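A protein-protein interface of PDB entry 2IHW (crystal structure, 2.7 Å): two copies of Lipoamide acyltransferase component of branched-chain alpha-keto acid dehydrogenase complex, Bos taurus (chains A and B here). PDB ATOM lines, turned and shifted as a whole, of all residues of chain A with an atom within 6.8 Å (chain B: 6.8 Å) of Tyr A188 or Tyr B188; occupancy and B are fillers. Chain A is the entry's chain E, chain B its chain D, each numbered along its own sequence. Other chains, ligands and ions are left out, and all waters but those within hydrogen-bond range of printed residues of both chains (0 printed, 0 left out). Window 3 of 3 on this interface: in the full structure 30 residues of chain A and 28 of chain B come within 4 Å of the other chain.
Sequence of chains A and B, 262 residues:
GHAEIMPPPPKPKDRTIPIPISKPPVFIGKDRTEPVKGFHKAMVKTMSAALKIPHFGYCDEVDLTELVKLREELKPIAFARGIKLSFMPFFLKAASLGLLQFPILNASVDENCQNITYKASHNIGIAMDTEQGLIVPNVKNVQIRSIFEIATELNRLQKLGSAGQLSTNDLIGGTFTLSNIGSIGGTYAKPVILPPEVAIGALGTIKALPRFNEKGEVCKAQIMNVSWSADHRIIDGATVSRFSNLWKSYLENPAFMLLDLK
Cys A59 touches Gly B186, but with the chains exchanged Gly A186 does not touch Cys B59 (14.7 Å).
Asp A60 touches Thr B187, but with the chains exchanged Thr A187 does not touch Asp B60 (12.4 Å).
Tyr A188 touches Thr B187, but with the chains exchanged Thr A187 does not touch Tyr B188 (7.5 Å).
Tyr B188 touches its own counterpart, Tyr A188.
16 positions are printed for both chains.
Of the 12 pairs that touch across the chains among the printed residues, 1 has its exchanged pair printed and touching as well.
Of the 17 printed residues of chain B, 6 touch a printed residue of chain A.
Printed residues of chain B that touch a printed residue of chain A: Ile B181, Gly B186, Thr B187, Tyr B188, Ala B189 and Lys B190.
Hydrophobic or aromatic side chains of chain B that line the printed part of chain A: Ile B181, Tyr B188 and Ala B189.
Among the printed residues, no Asp or Glu carboxylate lies within 4 Å of a Lys or Arg side-chain nitrogen of the other chain.
Tyr A188 touches just these residues of chain B: Thr B187 (2.8 Å) and Tyr B188 (3.5 Å).
Tyr B188 touches three residues of chain A.
Printed residues of chain B within 4 Å of Gly A57: Ala B189 and Lys B190.
Printed residues of chain B within 4 Å of Cys A59: Gly B186 (3.2 Å), Thr B187 (2.8 Å) and Tyr B188 (2.7 Å).
Of the printed residues of chain A, Gly B186 touches Tyr A58 (2.9 Å), Cys A59 (3.2 Å) and Asp A60 (3.4 Å).
Of the printed residues of chain B, Asp A60 touches Gly B186 and Thr B187.
Of the printed residues of chain B, Tyr A58 touches Ile B181, Gly B186 and Tyr B188.
Ala B202 touches none of the printed residues of chain A.
Ile A181 touches none of the printed residues of chain B.
The nearest residue of chain B that does not touch Tyr A188 is Asn B225 (5.3 Å).
The nearest residue of chain A that does not touch Tyr B188 is Gly A57 (4.7 Å).
The nearest printed residue of chain B that does not touch Tyr A58 is Ala B189 (4.3 Å).
The side-chain hydroxyl (OH) of Tyr A58 sits at hydrogen-bond distance from the backbone NH (N) of Gly B186 (2.9 Å).
The side-chain carboxylate of Asp A60 sits at hydrogen-bond distance from the backbone NH of Gly B186 (3.4 Å).
O of Cys A59 lies within hydrogen-bond range of N of Thr B187, at 2.8 Å.
The side-chain hydroxyl of Tyr A188 sits at hydrogen-bond distance from the side-chain hydroxyl of Thr B187 (2.8 Å).
O of Tyr B188 lies within hydrogen-bond range of N of Cys A59 (2.7 Å).
The backbone carbonyl oxygen (O) of Gly A57 lies within hydrogen-bond range of the backbone NH (N) of Lys B190, at 2.5 Å.
The side-chain amide nitrogen of Asn B225 lies within hydrogen-bond range of the side-chain hydroxyl of Tyr B188 (3.1 Å).
The backbone NH of Ala B189 sits at hydrogen-bond distance from the side-chain hydroxyl of Ser B227.
The side-chain sulfur of Cys A59 is in hydrogen-bond range of the side-chain hydroxyl of Ser A227 (3.1 Å).
The backbone carbonyl oxygen of Val A226 lies within hydrogen-bond range of the backbone NH of Asp A60 (2.9 Å).
OH of Tyr A188 is in hydrogen-bond range of ND2 of Asn A225 (2.9 Å).
Among the printed residues, merely in contact across the chains: Gly A57 with Ala B189 (3.0 Å), Tyr A58 with Ile B181 (3.9 Å), Tyr A58 with Tyr B188 (3.8 Å), Cys A59 with Gly B186 (3.2 Å), Asp A60 with Thr B187 (3.6 Å) and Tyr A188 with Tyr B188 (3.5 Å).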
ATOM      1  N   GLY A  57      29.767  35.484 -23.164  1.00  0.00           N
ATOM      2  CA  GLY A  57      29.923  34.082 -23.418  1.00  0.00           C
ATOM      3  C   GLY A  57      28.637  33.385 -23.152  1.00  0.00           C
ATOM      4  O   GLY A  57      28.112  33.481 -22.028  1.00  0.00           O
ATOM      5  N   TYR A  58      28.128  32.688 -24.183  1.00  0.00           N
ATOM      6  CA  TYR A  58      26.995  31.789 -24.021  1.00  0.00           C
ATOM      7  C   TYR A  58      27.256  30.323 -24.446  1.00  0.00           C
ATOM      8  O   TYR A  58      27.565  30.042 -25.626  1.00  0.00           O
ATOM      9  CB  TYR A  58      25.840  32.333 -24.833  1.00  0.00           C
ATOM     10  CG  TYR A  58      24.649  31.417 -24.916  1.00  0.00           C
ATOM     11  CD1 TYR A  58      24.551  30.432 -25.894  1.00  0.00           C
ATOM     12  CD2 TYR A  58      23.614  31.536 -23.998  1.00  0.00           C
ATOM     13  CE1 TYR A  58      23.409  29.594 -25.951  1.00  0.00           C
ATOM     14  CE2 TYR A  58      22.479  30.709 -24.055  1.00  0.00           C
ATOM     15  CZ  TYR A  58      22.394  29.768 -25.032  1.00  0.00           C
ATOM     16  OH  TYR A  58      21.274  28.989 -25.043  1.00  0.00           O
ATOM     17  N   CYS A  59      27.068  29.376 -23.536  1.00  0.00           N
ATOM     18  CA  CYS A  59      27.357  27.983 -23.899  1.00  0.00           C
ATOM     19  C   CYS A  59      26.203  27.071 -23.785  1.00  0.00           C
ATOM     20  O   CYS A  59      25.252  27.371 -23.074  1.00  0.00           O
ATOM     21  CB  CYS A  59      28.392  27.422 -22.971  1.00  0.00           C
ATOM     22  SG  CYS A  59      29.820  28.364 -23.000  1.00  0.00           S
ATOM     23  N   ASP A  60      26.336  25.921 -24.434  1.00  0.00           N
ATOM     24  CA  ASP A  60      25.261  24.921 -24.459  1.00  0.00           C
ATOM     25  C   ASP A  60      25.780  23.513 -24.761  1.00  0.00           C
ATOM     26  O   ASP A  60      26.988  23.297 -24.912  1.00  0.00           O
ATOM     27  CB  ASP A  60      24.127  25.303 -25.454  1.00  0.00           C
ATOM     28  CG  ASP A  60      22.733  24.727 -25.039  1.00  0.00           C
ATOM     29  OD1 ASP A  60      22.659  23.831 -24.152  1.00  0.00           O
ATOM     30  OD2 ASP A  60      21.709  25.178 -25.596  1.00  0.00           O
ATOM     31  N   GLU A  61      24.862  22.552 -24.764  1.00  0.00           N
ATOM     32  CA  GLU A  61      25.167  21.202 -25.184  1.00  0.00           C
ATOM     33  C   GLU A  61      24.183  20.742 -26.225  1.00  0.00           C
ATOM     34  O   GLU A  61      23.011  21.063 -26.169  1.00  0.00           O
ATOM     35  CB  GLU A  61      25.237  20.252 -24.002  1.00  0.00           C
ATOM     36  CG  GLU A  61      24.021  19.521 -23.614  1.00  0.00           C
ATOM     37  CD  GLU A  61      24.405  18.391 -22.651  1.00  0.00           C
ATOM     38  OE1 GLU A  61      25.513  18.478 -22.049  1.00  0.00           O
ATOM     39  OE2 GLU A  61      23.642  17.401 -22.506  1.00  0.00           O
ATOM     40  N   ILE A 181      37.844  23.260 -31.885  1.00  0.00           N
ATOM     41  CA  ILE A 181      38.859  22.777 -30.941  1.00  0.00           C
ATOM     42  C   ILE A 181      38.673  21.299 -30.541  1.00  0.00           C
ATOM     43  O   ILE A 181      39.615  20.656 -30.047  1.00  0.00           O
ATOM     44  CB  ILE A 181      38.854  23.620 -29.655  1.00  0.00           C
ATOM     45  CG1 ILE A 181      37.660  23.208 -28.774  1.00  0.00           C
ATOM     46  CG2 ILE A 181      38.906  25.122 -30.018  1.00  0.00           C
ATOM     47  CD1 ILE A 181      37.609  23.865 -27.440  1.00  0.00           C
ATOM     48  N   GLY A 186      38.772  18.713 -25.428  1.00  0.00           N
ATOM     49  CA  GLY A 186      37.980  19.690 -24.682  1.00  0.00           C
ATOM     50  C   GLY A 186      36.465  19.699 -24.750  1.00  0.00           C
ATOM     51  O   GLY A 186      35.797  18.930 -25.486  1.00  0.00           O
ATOM     52  N   THR A 187      35.918  20.573 -23.927  1.00  0.00           N
ATOM     53  CA  THR A 187      34.487  20.657 -23.776  1.00  0.00           C
ATOM     54  C   THR A 187      34.039  22.078 -24.130  1.00  0.00           C
ATOM     55  O   THR A 187      33.753  22.335 -25.290  1.00  0.00           O
ATOM     56  CB  THR A 187      34.015  20.194 -22.363  1.00  0.00           C
ATOM     57  OG1 THR A 187      34.578  21.024 -21.328  1.00  0.00           O
ATOM     58  CG2 THR A 187      34.400  18.724 -22.123  1.00  0.00           C
ATOM     59  N   TYR A 188      34.016  22.991 -23.157  1.00  0.00           N
ATOM     60  CA  TYR A 188      33.597  24.378 -23.359  1.00  0.00           C
ATOM     61  C   TYR A 188      34.805  25.205 -23.550  1.00  0.00           C
ATOM     62  O   TYR A 188      35.910  24.824 -23.150  1.00  0.00           O
ATOM     63  CB  TYR A 188      32.870  24.915 -22.139  1.00  0.00           C
ATOM     64  CG  TYR A 188      31.514  24.318 -21.974  1.00  0.00           C
ATOM     65  CD1 TYR A 188      30.445  24.701 -22.818  1.00  0.00           C
ATOM     66  CD2 TYR A 188      31.270  23.365 -20.984  1.00  0.00           C
ATOM     67  CE1 TYR A 188      29.166  24.112 -22.672  1.00  0.00           C
ATOM     68  CE2 TYR A 188      29.994  22.803 -20.809  1.00  0.00           C
ATOM     69  CZ  TYR A 188      28.956  23.174 -21.657  1.00  0.00           C
ATOM     70  OH  TYR A 188      27.719  22.607 -21.498  1.00  0.00           O
ATOM     71  N   ALA A 189      34.621  26.381 -24.117  1.00  0.00           N
ATOM     72  CA  ALA A 189      35.787  27.228 -24.332  1.00  0.00           C
ATOM     73  C   ALA A 189      35.338  28.657 -24.225  1.00  0.00           C
ATOM     74  O   ALA A 189      34.149  28.931 -24.046  1.00  0.00           O
ATOM     75  CB  ALA A 189      36.378  26.948 -25.687  1.00  0.00           C
ATOM     76  N   LYS A 190      36.281  29.578 -24.298  1.00  0.00           N
ATOM     77  CA  LYS A 190      35.934  30.979 -24.392  1.00  0.00           C
ATOM     78  C   LYS A 190      36.704  31.462 -25.615  1.00  0.00           C
ATOM     79  O   LYS A 190      37.857  31.801 -25.508  1.00  0.00           O
ATOM     80  CB  LYS A 190      36.339  31.705 -23.109  1.00  0.00           C
ATOM     81  CG  LYS A 190      36.088  33.237 -23.133  1.00  0.00           C
ATOM     82  CD  LYS A 190      37.327  34.138 -23.603  1.00  0.00           C
ATOM     83  CE  LYS A 190      37.062  35.642 -23.327  1.00  0.00           C
ATOM     84  NZ  LYS A 190      38.096  36.597 -23.921  1.00  0.00           N
ATOM     85  N   PRO A 191      36.105  31.394 -26.805  1.00  0.00           N
ATOM     86  CA  PRO A 191      36.848  31.837 -27.946  1.00  0.00           C
ATOM     87  C   PRO A 191      36.903  33.353 -28.013  1.00  0.00           C
ATOM     88  O   PRO A 191      36.093  34.034 -27.351  1.00  0.00           O
ATOM     89  CB  PRO A 191      36.067  31.268 -29.091  1.00  0.00           C
ATOM     90  CG  PRO A 191      34.714  31.266 -28.616  1.00  0.00           C
ATOM     91  CD  PRO A 191      34.775  30.906 -27.183  1.00  0.00           C
ATOM     92  N   ALA A 202      33.078  27.997 -30.629  1.00  0.00           N
ATOM     93  CA  ALA A 202      34.038  26.937 -30.473  1.00  0.00           C
ATOM     94  C   ALA A 202      33.244  25.645 -30.242  1.00  0.00           C
ATOM     95  O   ALA A 202      32.290  25.625 -29.438  1.00  0.00           O
ATOM     96  CB  ALA A 202      34.958  27.223 -29.295  1.00  0.00           C
ATOM     97  N   GLY A 204      33.316  21.532 -29.120  1.00  0.00           N
ATOM     98  CA  GLY A 204      34.129  20.644 -28.355  1.00  0.00           C
ATOM     99  C   GLY A 204      34.046  19.248 -28.874  1.00  0.00           C
ATOM    100  O   GLY A 204      33.428  18.988 -29.917  1.00  0.00           O
ATOM    101  N   MET A 224      27.861  17.044 -27.655  1.00  0.00           N
ATOM    102  CA  MET A 224      28.903  17.999 -27.953  1.00  0.00           C
ATOM    103  C   MET A 224      28.570  19.340 -27.285  1.00  0.00           C
ATOM    104  O   MET A 224      27.403  19.783 -27.245  1.00  0.00           O
ATOM    105  CB  MET A 224      29.050  18.180 -29.444  1.00  0.00           C
ATOM    106  CG  MET A 224      30.248  19.012 -29.838  1.00  0.00           C
ATOM    107  SD  MET A 224      30.272  19.360 -31.612  1.00  0.00           S
ATOM    108  CE  MET A 224      28.943  20.614 -31.686  1.00  0.00           C
ATOM    109  N   ASN A 225      29.592  19.961 -26.721  1.00  0.00           N
ATOM    110  CA  ASN A 225      29.427  21.251 -26.153  1.00  0.00           C
ATOM    111  C   ASN A 225      29.712  22.316 -27.200  1.00  0.00           C
ATOM    112  O   ASN A 225      30.592  22.146 -28.045  1.00  0.00           O
ATOM    113  CB  ASN A 225      30.320  21.353 -24.918  1.00  0.00           C
ATOM    114  CG  ASN A 225      29.891  20.384 -23.842  1.00  0.00           C
ATOM    115  OD1 ASN A 225      30.590  19.431 -23.541  1.00  0.00           O
ATOM    116  ND2 ASN A 225      28.725  20.605 -23.275  1.00  0.00           N
ATOM    117  N   VAL A 226      28.961  23.409 -27.148  1.00  0.00           N
ATOM    118  CA  VAL A 226      29.241  24.574 -27.982  1.00  0.00           C
ATOM    119  C   VAL A 226      29.449  25.793 -27.103  1.00  0.00           C
ATOM    120  O   VAL A 226      28.713  25.962 -26.114  1.00  0.00           O
ATOM    121  CB  VAL A 226      28.094  24.855 -28.989  1.00  0.00           C
ATOM    122  CG1 VAL A 226      26.783  25.125 -28.266  1.00  0.00           C
ATOM    123  CG2 VAL A 226      28.452  26.037 -29.885  1.00  0.00           C
ATOM    124  N   SER A 227      30.410  26.651 -27.479  1.00  0.00           N
ATOM    125  CA  SER A 227      30.629  27.920 -26.777  1.00  0.00           C
ATOM    126  C   SER A 227      30.615  29.101 -27.728  1.00  0.00           C
ATOM    127  O   SER A 227      31.422  29.161 -28.667  1.00  0.00           O
ATOM    128  CB  SER A 227      31.961  27.889 -26.059  1.00  0.00           C
ATOM    129  OG  SER A 227      31.863  27.056 -24.935  1.00  0.00           O
ATOM    130  N   CYS B  59      31.945  28.926 -11.994  1.00  0.00           N
ATOM    131  CA  CYS B  59      30.734  28.247 -12.417  1.00  0.00           C
ATOM    132  C   CYS B  59      30.549  27.018 -11.632  1.00  0.00           C
ATOM    133  O   CYS B  59      31.522  26.482 -11.086  1.00  0.00           O
ATOM    134  CB  CYS B  59      30.864  27.791 -13.860  1.00  0.00           C
ATOM    135  SG  CYS B  59      31.141  29.154 -14.879  1.00  0.00           S
ATOM    136  N   ASP B  60      29.303  26.559 -11.595  1.00  0.00           N
ATOM    137  CA  ASP B  60      28.997  25.353 -10.877  1.00  0.00           C
ATOM    138  C   ASP B  60      27.662  24.787 -11.335  1.00  0.00           C
ATOM    139  O   ASP B  60      27.007  25.344 -12.218  1.00  0.00           O
ATOM    140  CB  ASP B  60      29.073  25.619  -9.362  1.00  0.00           C
ATOM    141  CG  ASP B  60      29.126  24.334  -8.510  1.00  0.00           C
ATOM    142  OD1 ASP B  60      29.378  23.201  -8.989  1.00  0.00           O
ATOM    143  OD2 ASP B  60      28.892  24.478  -7.306  1.00  0.00           O
ATOM    144  N   GLU B  61      27.289  23.666 -10.729  1.00  0.00           N
ATOM    145  CA  GLU B  61      26.161  22.833 -11.097  1.00  0.00           C
ATOM    146  C   GLU B  61      25.265  22.777  -9.875  1.00  0.00           C
ATOM    147  O   GLU B  61      25.767  22.606  -8.745  1.00  0.00           O
ATOM    148  CB  GLU B  61      26.669  21.429 -11.455  1.00  0.00           C
ATOM    149  CG  GLU B  61      25.573  20.420 -11.482  1.00  0.00           C
ATOM    150  CD  GLU B  61      25.987  19.063 -12.009  1.00  0.00           C
ATOM    151  OE1 GLU B  61      26.474  19.008 -13.165  1.00  0.00           O
ATOM    152  OE2 GLU B  61      25.794  18.043 -11.279  1.00  0.00           O
ATOM    153  N   ILE B 181      19.281  33.268 -18.555  1.00  0.00           N
ATOM    154  CA  ILE B 181      19.508  32.901 -19.942  1.00  0.00           C
ATOM    155  C   ILE B 181      18.733  31.612 -20.300  1.00  0.00           C
ATOM    156  O   ILE B 181      18.309  31.396 -21.450  1.00  0.00           O
ATOM    157  CB  ILE B 181      21.067  32.740 -20.229  1.00  0.00           C
ATOM    158  CG1 ILE B 181      21.647  31.453 -19.592  1.00  0.00           C
ATOM    159  CG2 ILE B 181      21.871  33.993 -19.811  1.00  0.00           C
ATOM    160  CD1 ILE B 181      22.981  30.984 -20.196  1.00  0.00           C
ATOM    161  N   GLY B 186      20.702  27.132 -22.942  1.00  0.00           N
ATOM    162  CA  GLY B 186      22.095  27.267 -22.533  1.00  0.00           C
ATOM    163  C   GLY B 186      22.412  26.554 -21.247  1.00  0.00           C
ATOM    164  O   GLY B 186      21.514  26.153 -20.503  1.00  0.00           O
ATOM    165  N   THR B 187      23.699  26.371 -20.987  1.00  0.00           N
ATOM    166  CA  THR B 187      24.153  25.767 -19.750  1.00  0.00           C
ATOM    167  C   THR B 187      25.023  26.811 -19.108  1.00  0.00           C
ATOM    168  O   THR B 187      24.552  27.520 -18.227  1.00  0.00           O
ATOM    169  CB  THR B 187      24.979  24.517 -19.973  1.00  0.00           C
ATOM    170  OG1 THR B 187      25.975  24.782 -20.978  1.00  0.00           O
ATOM    171  CG2 THR B 187      24.098  23.397 -20.410  1.00  0.00           C
ATOM    172  N   TYR B 188      26.270  26.946 -19.546  1.00  0.00           N
ATOM    173  CA  TYR B 188      27.227  27.867 -18.897  1.00  0.00           C
ATOM    174  C   TYR B 188      27.294  29.110 -19.716  1.00  0.00           C
ATOM    175  O   TYR B 188      26.846  29.117 -20.817  1.00  0.00           O
ATOM    176  CB  TYR B 188      28.615  27.265 -18.750  1.00  0.00           C
ATOM    177  CG  TYR B 188      28.688  26.173 -17.741  1.00  0.00           C
ATOM    178  CD1 TYR B 188      28.569  26.461 -16.390  1.00  0.00           C
ATOM    179  CD2 TYR B 188      28.879  24.828 -18.117  1.00  0.00           C
ATOM    180  CE1 TYR B 188      28.605  25.435 -15.421  1.00  0.00           C
ATOM    181  CE2 TYR B 188      28.962  23.822 -17.170  1.00  0.00           C
ATOM    182  CZ  TYR B 188      28.822  24.139 -15.819  1.00  0.00           C
ATOM    183  OH  TYR B 188      28.872  23.194 -14.823  1.00  0.00           O
ATOM    184  N   ALA B 189      27.873  30.161 -19.174  1.00  0.00           N
ATOM    185  CA  ALA B 189      27.853  31.470 -19.813  1.00  0.00           C
ATOM    186  C   ALA B 189      28.931  32.316 -19.131  1.00  0.00           C
ATOM    187  O   ALA B 189      29.387  31.955 -18.020  1.00  0.00           O
ATOM    188  CB  ALA B 189      26.504  32.094 -19.600  1.00  0.00           C
ATOM    189  N   LYS B 190      29.325  33.402 -19.797  1.00  0.00           N
ATOM    190  CA  LYS B 190      30.254  34.404 -19.295  1.00  0.00           C
ATOM    191  C   LYS B 190      29.465  35.718 -19.338  1.00  0.00           C
ATOM    192  O   LYS B 190      29.447  36.440 -20.383  1.00  0.00           O
ATOM    193  CB  LYS B 190      31.462  34.485 -20.232  1.00  0.00           C
ATOM    194  CG  LYS B 190      32.599  35.516 -19.878  1.00  0.00           C
ATOM    195  CD  LYS B 190      32.436  37.029 -20.303  1.00  0.00           C
ATOM    196  CE  LYS B 190      33.808  37.732 -20.285  1.00  0.00           C
ATOM    197  NZ  LYS B 190      33.781  39.258 -20.275  1.00  0.00           N
ATOM    198  N   PRO B 191      28.703  35.999 -18.264  1.00  0.00           N
ATOM    199  CA  PRO B 191      27.926  37.245 -18.251  1.00  0.00           C
ATOM    200  C   PRO B 191      28.833  38.478 -18.077  1.00  0.00           C
ATOM    201  O   PRO B 191      29.923  38.368 -17.514  1.00  0.00           O
ATOM    202  CB  PRO B 191      27.039  37.086 -17.012  1.00  0.00           C
ATOM    203  CG  PRO B 191      27.829  36.130 -16.072  1.00  0.00           C
ATOM    204  CD  PRO B 191      28.491  35.182 -17.042  1.00  0.00           C
ATOM    205  N   ALA B 202      24.597  34.070 -14.090  1.00  0.00           N
ATOM    206  CA  ALA B 202      23.705  33.636 -15.158  1.00  0.00           C
ATOM    207  C   ALA B 202      23.135  32.254 -14.820  1.00  0.00           C
ATOM    208  O   ALA B 202      23.831  31.391 -14.266  1.00  0.00           O
ATOM    209  CB  ALA B 202      24.396  33.661 -16.463  1.00  0.00           C
ATOM    210  N   GLY B 204      21.230  28.880 -16.272  1.00  0.00           N
ATOM    211  CA  GLY B 204      21.071  28.041 -17.431  1.00  0.00           C
ATOM    212  C   GLY B 204      19.770  27.299 -17.331  1.00  0.00           C
ATOM    213  O   GLY B 204      18.989  27.552 -16.429  1.00  0.00           O
ATOM    214  N   LYS B 207      17.630  20.918 -16.714  1.00  0.00           N
ATOM    215  CA  LYS B 207      17.688  19.728 -17.517  1.00  0.00           C
ATOM    216  C   LYS B 207      17.768  18.524 -16.586  1.00  0.00           C
ATOM    217  O   LYS B 207      18.517  18.517 -15.591  1.00  0.00           O
ATOM    218  CB  LYS B 207      18.905  19.792 -18.452  1.00  0.00           C
ATOM    219  CG  LYS B 207      18.522  19.927 -19.966  1.00  0.00           C
ATOM    220  CD  LYS B 207      19.520  19.251 -21.001  1.00  0.00           C
ATOM    221  CE  LYS B 207      20.656  20.243 -21.418  1.00  0.00           C
ATOM    222  NZ  LYS B 207      21.501  20.679 -20.265  1.00  0.00           N
ATOM    223  N   MET B 224      20.739  22.371 -12.964  1.00  0.00           N
ATOM    224  CA  MET B 224      20.896  23.668 -13.548  1.00  0.00           C
ATOM    225  C   MET B 224      22.369  24.165 -13.384  1.00  0.00           C
ATOM    226  O   MET B 224      23.003  23.984 -12.334  1.00  0.00           O
ATOM    227  CB  MET B 224      19.911  24.636 -12.907  1.00  0.00           C
ATOM    228  CG  MET B 224      19.561  25.816 -13.789  1.00  0.00           C
ATOM    229  SD  MET B 224      19.063  27.313 -12.889  1.00  0.00           S
ATOM    230  CE  MET B 224      20.306  27.422 -11.612  1.00  0.00           C
ATOM    231  N   ASN B 225      22.904  24.775 -14.430  1.00  0.00           N
ATOM    232  CA  ASN B 225      24.173  25.431 -14.327  1.00  0.00           C
ATOM    233  C   ASN B 225      24.051  26.913 -13.920  1.00  0.00           C
ATOM    234  O   ASN B 225      23.056  27.570 -14.254  1.00  0.00           O
ATOM    235  CB  ASN B 225      24.901  25.255 -15.661  1.00  0.00           C
ATOM    236  CG  ASN B 225      25.223  23.776 -15.948  1.00  0.00           C
ATOM    237  OD1 ASN B 225      24.953  23.298 -17.031  1.00  0.00           O
ATOM    238  ND2 ASN B 225      25.786  23.058 -14.965  1.00  0.00           N
ATOM    239  N   VAL B 226      25.033  27.418 -13.165  1.00  0.00           N
ATOM    240  CA  VAL B 226      25.147  28.858 -12.860  1.00  0.00           C
ATOM    241  C   VAL B 226      26.563  29.341 -13.142  1.00  0.00           C
ATOM    242  O   VAL B 226      27.519  28.658 -12.789  1.00  0.00           O
ATOM    243  CB  VAL B 226      24.827  29.166 -11.365  1.00  0.00           C
ATOM    244  CG1 VAL B 226      25.777  28.415 -10.392  1.00  0.00           C
ATOM    245  CG2 VAL B 226      24.897  30.638 -11.117  1.00  0.00           C
ATOM    246  N   SER B 227      26.696  30.509 -13.746  1.00  0.00           N
ATOM    247  CA  SER B 227      28.014  31.104 -14.012  1.00  0.00           C
ATOM    248  C   SER B 227      28.078  32.497 -13.385  1.00  0.00           C
ATOM    249  O   SER B 227      27.304  33.391 -13.754  1.00  0.00           O
ATOM    250  CB  SER B 227      28.238  31.253 -15.515  1.00  0.00           C
ATOM    251  OG  SER B 227      27.935  30.049 -16.214  1.00  0.00           O
